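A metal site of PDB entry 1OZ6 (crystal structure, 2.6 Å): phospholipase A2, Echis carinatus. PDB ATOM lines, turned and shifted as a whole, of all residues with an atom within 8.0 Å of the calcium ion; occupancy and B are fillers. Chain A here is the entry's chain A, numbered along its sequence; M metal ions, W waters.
The calcium ion is bound by O of Tyr 27 (2.5 Å), water W1 (2.5 Å), O of Gly 31 (2.6 Å), OD2 of Asp 48 (2.7 Å) and O of Gly 29 (2.7 Å). The calcium ion has five donor atoms within binding distance. Slightly farther from the calcium ion lies the side-chain carboxylate (OD1) of Asp 48 (2.9 Å).
The backbone NH (N) of Tyr 27 is in hydrogen-bond range of the side-chain carboxylate (OD1) of Asp 41, at 2.9 Å. The side-chain sulfur (SG) of Cys 28 is disulfide-bonded to the side-chain sulfur (SG) of Cys 44 (2.0 Å).
Within 4 Å of the calcium ion: Tyr 27, Gly 29, Gly 31 and Asp 48.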
ATOM      1  N   TYR A  21     -10.755 -18.611 -10.779  1.00  0.00           N
ATOM      2  CA  TYR A  21      -9.733 -17.577 -10.743  1.00  0.00           C
ATOM      3  C   TYR A  21      -8.962 -17.436 -12.040  1.00  0.00           C
ATOM      4  O   TYR A  21      -8.156 -16.523 -12.191  1.00  0.00           O
ATOM      5  CB  TYR A  21      -8.755 -17.864  -9.609  1.00  0.00           C
ATOM      6  CG  TYR A  21      -9.373 -17.860  -8.228  1.00  0.00           C
ATOM      7  CD1 TYR A  21      -9.616 -16.661  -7.556  1.00  0.00           C
ATOM      8  CD2 TYR A  21      -9.752 -19.054  -7.612  1.00  0.00           C
ATOM      9  CE1 TYR A  21     -10.209 -16.654  -6.302  1.00  0.00           C
ATOM     10  CE2 TYR A  21     -10.339 -19.056  -6.359  1.00  0.00           C
ATOM     11  CZ  TYR A  21     -10.567 -17.856  -5.704  1.00  0.00           C
ATOM     12  OH  TYR A  21     -11.157 -17.858  -4.465  1.00  0.00           O
ATOM     13  N   GLY A  22      -9.221 -18.337 -12.991  1.00  0.00           N
ATOM     14  CA  GLY A  22      -8.530 -18.276 -14.265  1.00  0.00           C
ATOM     15  C   GLY A  22      -8.694 -16.977 -15.022  1.00  0.00           C
ATOM     16  O   GLY A  22      -7.810 -16.586 -15.784  1.00  0.00           O
ATOM     17  N   TYR A  24     -10.403 -14.047 -13.330  1.00  0.00           N
ATOM     18  CA  TYR A  24     -10.970 -13.123 -12.348  1.00  0.00           C
ATOM     19  C   TYR A  24     -10.270 -11.772 -12.290  1.00  0.00           C
ATOM     20  O   TYR A  24      -9.032 -11.676 -12.288  1.00  0.00           O
ATOM     21  CB  TYR A  24     -10.945 -13.796 -10.971  1.00  0.00           C
ATOM     22  CG  TYR A  24     -11.826 -13.146  -9.932  1.00  0.00           C
ATOM     23  CD1 TYR A  24     -11.372 -12.074  -9.167  1.00  0.00           C
ATOM     24  CD2 TYR A  24     -13.107 -13.652  -9.671  1.00  0.00           C
ATOM     25  CE1 TYR A  24     -12.175 -11.511  -8.168  1.00  0.00           C
ATOM     26  CE2 TYR A  24     -13.911 -13.101  -8.679  1.00  0.00           C
ATOM     27  CZ  TYR A  24     -13.442 -12.028  -7.932  1.00  0.00           C
ATOM     28  OH  TYR A  24     -14.236 -11.481  -6.949  1.00  0.00           O
ATOM     29  N   CYS A  26      -8.654  -8.067 -12.932  1.00  0.00           N
ATOM     30  CA  CYS A  26      -7.643  -7.577 -13.860  1.00  0.00           C
ATOM     31  C   CYS A  26      -6.289  -8.262 -13.709  1.00  0.00           C
ATOM     32  O   CYS A  26      -5.419  -8.096 -14.554  1.00  0.00           O
ATOM     33  CB  CYS A  26      -7.438  -6.077 -13.668  1.00  0.00           C
ATOM     34  SG  CYS A  26      -8.927  -5.061 -13.871  1.00  0.00           S
ATOM     35  N   TYR A  27      -6.116  -9.049 -12.657  1.00  0.00           N
ATOM     36  CA  TYR A  27      -4.802  -9.669 -12.481  1.00  0.00           C
ATOM     37  C   TYR A  27      -4.782 -11.168 -12.236  1.00  0.00           C
ATOM     38  O   TYR A  27      -3.703 -11.747 -12.205  1.00  0.00           O
ATOM     39  CB  TYR A  27      -4.093  -8.954 -11.321  1.00  0.00           C
ATOM     40  CG  TYR A  27      -3.703  -7.509 -11.593  1.00  0.00           C
ATOM     41  CD1 TYR A  27      -4.615  -6.473 -11.395  1.00  0.00           C
ATOM     42  CD2 TYR A  27      -2.432  -7.180 -12.064  1.00  0.00           C
ATOM     43  CE1 TYR A  27      -4.279  -5.150 -11.652  1.00  0.00           C
ATOM     44  CE2 TYR A  27      -2.079  -5.857 -12.324  1.00  0.00           C
ATOM     45  CZ  TYR A  27      -3.009  -4.845 -12.124  1.00  0.00           C
ATOM     46  OH  TYR A  27      -2.672  -3.534 -12.374  1.00  0.00           O
ATOM     47  N   CYS A  28      -5.922 -11.821 -12.050  1.00  0.00           N
ATOM     48  CA  CYS A  28      -5.894 -13.255 -11.803  1.00  0.00           C
ATOM     49  C   CYS A  28      -5.647 -14.050 -13.076  1.00  0.00           C
ATOM     50  O   CYS A  28      -4.936 -15.050 -13.052  1.00  0.00           O
ATOM     51  CB  CYS A  28      -7.187 -13.729 -11.129  1.00  0.00           C
ATOM     52  SG  CYS A  28      -7.402 -13.106  -9.427  1.00  0.00           S
ATOM     53  N   GLY A  29      -6.218 -13.598 -14.182  1.00  0.00           N
ATOM     54  CA  GLY A  29      -6.003 -14.269 -15.457  1.00  0.00           C
ATOM     55  C   GLY A  29      -4.554 -14.077 -15.857  1.00  0.00           C
ATOM     56  O   GLY A  29      -3.721 -13.796 -15.009  1.00  0.00           O
ATOM     57  N   TRP A  30      -4.241 -14.235 -17.147  1.00  0.00           N
ATOM     58  CA  TRP A  30      -2.866 -14.058 -17.600  1.00  0.00           C
ATOM     59  C   TRP A  30      -2.659 -12.598 -17.950  1.00  0.00           C
ATOM     60  O   TRP A  30      -3.520 -11.970 -18.574  1.00  0.00           O
ATOM     61  CB  TRP A  30      -2.586 -14.921 -18.840  1.00  0.00           C
ATOM     62  CG  TRP A  30      -1.131 -14.948 -19.204  1.00  0.00           C
ATOM     63  CD1 TRP A  30      -0.186 -15.801 -18.708  1.00  0.00           C
ATOM     64  CD2 TRP A  30      -0.449 -14.033 -20.067  1.00  0.00           C
ATOM     65  NE1 TRP A  30       1.056 -15.474 -19.210  1.00  0.00           N
ATOM     66  CE2 TRP A  30       0.920 -14.397 -20.049  1.00  0.00           C
ATOM     67  CE3 TRP A  30      -0.852 -12.946 -20.854  1.00  0.00           C
ATOM     68  CZ2 TRP A  30       1.891 -13.699 -20.793  1.00  0.00           C
ATOM     69  CZ3 TRP A  30       0.115 -12.253 -21.590  1.00  0.00           C
ATOM     70  CH2 TRP A  30       1.464 -12.645 -21.550  1.00  0.00           C
ATOM     71  N   GLY A  31      -1.508 -12.045 -17.562  1.00  0.00           N
ATOM     72  CA  GLY A  31      -1.286 -10.665 -17.882  1.00  0.00           C
ATOM     73  C   GLY A  31      -1.785  -9.823 -16.723  1.00  0.00           C
ATOM     74  O   GLY A  31      -1.710 -10.243 -15.576  1.00  0.00           O
ATOM     75  N   GLY A  32      -2.302  -8.639 -17.019  1.00  0.00           N
ATOM     76  CA  GLY A  32      -2.821  -7.808 -15.943  1.00  0.00           C
ATOM     77  C   GLY A  32      -2.425  -6.352 -16.036  1.00  0.00           C
ATOM     78  O   GLY A  32      -1.278  -6.024 -16.336  1.00  0.00           O
ATOM     79  N   GLN A  33      -3.383  -5.478 -15.775  1.00  0.00           N
ATOM     80  CA  GLN A  33      -3.176  -4.035 -15.810  1.00  0.00           C
ATOM     81  C   GLN A  33      -4.402  -3.397 -15.181  1.00  0.00           C
ATOM     82  O   GLN A  33      -5.372  -4.091 -14.890  1.00  0.00           O
ATOM     83  CB  GLN A  33      -3.055  -3.556 -17.259  1.00  0.00           C
ATOM     84  CG  GLN A  33      -4.271  -3.869 -18.110  1.00  0.00           C
ATOM     85  CD  GLN A  33      -4.132  -3.360 -19.531  1.00  0.00           C
ATOM     86  OE1 GLN A  33      -3.253  -3.772 -20.269  1.00  0.00           O
ATOM     87  NE2 GLN A  33      -5.028  -2.457 -19.918  1.00  0.00           N
ATOM     88  N   ASP A  41      -8.712  -9.897  -6.268  1.00  0.00           N
ATOM     89  CA  ASP A  41      -7.962  -9.394  -7.425  1.00  0.00           C
ATOM     90  C   ASP A  41      -6.615  -8.843  -6.984  1.00  0.00           C
ATOM     91  O   ASP A  41      -5.607  -9.038  -7.650  1.00  0.00           O
ATOM     92  CB  ASP A  41      -8.792  -8.320  -8.143  1.00  0.00           C
ATOM     93  CG  ASP A  41      -8.326  -8.055  -9.568  1.00  0.00           C
ATOM     94  OD1 ASP A  41      -7.658  -8.917 -10.168  1.00  0.00           O
ATOM     95  OD2 ASP A  41      -8.658  -6.975 -10.109  1.00  0.00           O
ATOM     96  N   CYS A  44      -4.035 -11.450  -6.561  1.00  0.00           N
ATOM     97  CA  CYS A  44      -3.444 -11.840  -7.838  1.00  0.00           C
ATOM     98  C   CYS A  44      -2.443 -10.824  -8.345  1.00  0.00           C
ATOM     99  O   CYS A  44      -1.579 -11.138  -9.153  1.00  0.00           O
ATOM    100  CB  CYS A  44      -4.539 -12.064  -8.891  1.00  0.00           C
ATOM    101  SG  CYS A  44      -5.604 -13.502  -8.556  1.00  0.00           S
ATOM    102  N   LEU A  45      -2.580  -9.581  -7.882  1.00  0.00           N
ATOM    103  CA  LEU A  45      -1.671  -8.510  -8.285  1.00  0.00           C
ATOM    104  C   LEU A  45      -0.337  -8.857  -7.643  1.00  0.00           C
ATOM    105  O   LEU A  45       0.636  -9.157  -8.324  1.00  0.00           O
ATOM    106  CB  LEU A  45      -2.179  -7.172  -7.747  1.00  0.00           C
ATOM    107  CG  LEU A  45      -1.476  -5.861  -8.152  1.00  0.00           C
ATOM    108  CD1 LEU A  45      -2.299  -4.686  -7.651  1.00  0.00           C
ATOM    109  CD2 LEU A  45      -0.071  -5.814  -7.570  1.00  0.00           C
ATOM    110  N   HIS A  47       0.862 -11.428  -6.415  1.00  0.00           N
ATOM    111  CA  HIS A  47       1.465 -12.660  -6.926  1.00  0.00           C
ATOM    112  C   HIS A  47       2.223 -12.359  -8.218  1.00  0.00           C
ATOM    113  O   HIS A  47       3.341 -12.849  -8.425  1.00  0.00           O
ATOM    114  CB  HIS A  47       0.374 -13.719  -7.160  1.00  0.00           C
ATOM    115  CG  HIS A  47       0.900 -15.088  -7.444  1.00  0.00           C
ATOM    116  ND1 HIS A  47       0.984 -15.603  -8.723  1.00  0.00           N
ATOM    117  CD2 HIS A  47       1.377 -16.049  -6.618  1.00  0.00           C
ATOM    118  CE1 HIS A  47       1.494 -16.822  -8.672  1.00  0.00           C
ATOM    119  NE2 HIS A  47       1.733 -17.119  -7.409  1.00  0.00           N
ATOM    120  N   ASP A  48       1.638 -11.524  -9.077  1.00  0.00           N
ATOM    121  CA  ASP A  48       2.276 -11.126 -10.336  1.00  0.00           C
ATOM    122  C   ASP A  48       3.601 -10.431 -10.047  1.00  0.00           C
ATOM    123  O   ASP A  48       4.624 -10.774 -10.632  1.00  0.00           O
ATOM    124  CB  ASP A  48       1.382 -10.158 -11.100  1.00  0.00           C
ATOM    125  CG  ASP A  48       0.273 -10.865 -11.848  1.00  0.00           C
ATOM    126  OD1 ASP A  48      -0.143 -11.965 -11.436  1.00  0.00           O
ATOM    127  OD2 ASP A  48      -0.203 -10.295 -12.856  1.00  0.00           O
ATOM    128  N   CYS A  49       3.570  -9.443  -9.157  1.00  0.00           N
ATOM    129  CA  CYS A  49       4.784  -8.711  -8.798  1.00  0.00           C
ATOM    130  C   CYS A  49       5.801  -9.665  -8.212  1.00  0.00           C
ATOM    131  O   CYS A  49       7.004  -9.519  -8.424  1.00  0.00           O
ATOM    132  CB  CYS A  49       4.462  -7.634  -7.776  1.00  0.00           C
ATOM    133  SG  CYS A  49       3.542  -6.178  -8.384  1.00  0.00           S
ATOM    134  N   TYR A  51       6.208 -12.755  -8.980  1.00  0.00           N
ATOM    135  CA  TYR A  51       6.808 -13.519 -10.073  1.00  0.00           C
ATOM    136  C   TYR A  51       7.878 -12.773 -10.859  1.00  0.00           C
ATOM    137  O   TYR A  51       8.818 -13.381 -11.345  1.00  0.00           O
ATOM    138  CB  TYR A  51       5.723 -14.031 -11.022  1.00  0.00           C
ATOM    139  CG  TYR A  51       5.244 -15.423 -10.696  1.00  0.00           C
ATOM    140  CD1 TYR A  51       5.453 -15.981  -9.428  1.00  0.00           C
ATOM    141  CD2 TYR A  51       4.563 -16.179 -11.641  1.00  0.00           C
ATOM    142  CE1 TYR A  51       4.998 -17.259  -9.113  1.00  0.00           C
ATOM    143  CE2 TYR A  51       4.090 -17.468 -11.330  1.00  0.00           C
ATOM    144  CZ  TYR A  51       4.311 -17.994 -10.063  1.00  0.00           C
ATOM    145  OH  TYR A  51       3.830 -19.230  -9.741  1.00  0.00           O
HETATM  146 CA    CA M   1      -1.885 -12.186 -13.803  1.00  0.00          CA
HETATM  147  O   HOH W   1      -1.959 -14.687 -13.337  1.00  0.00           O
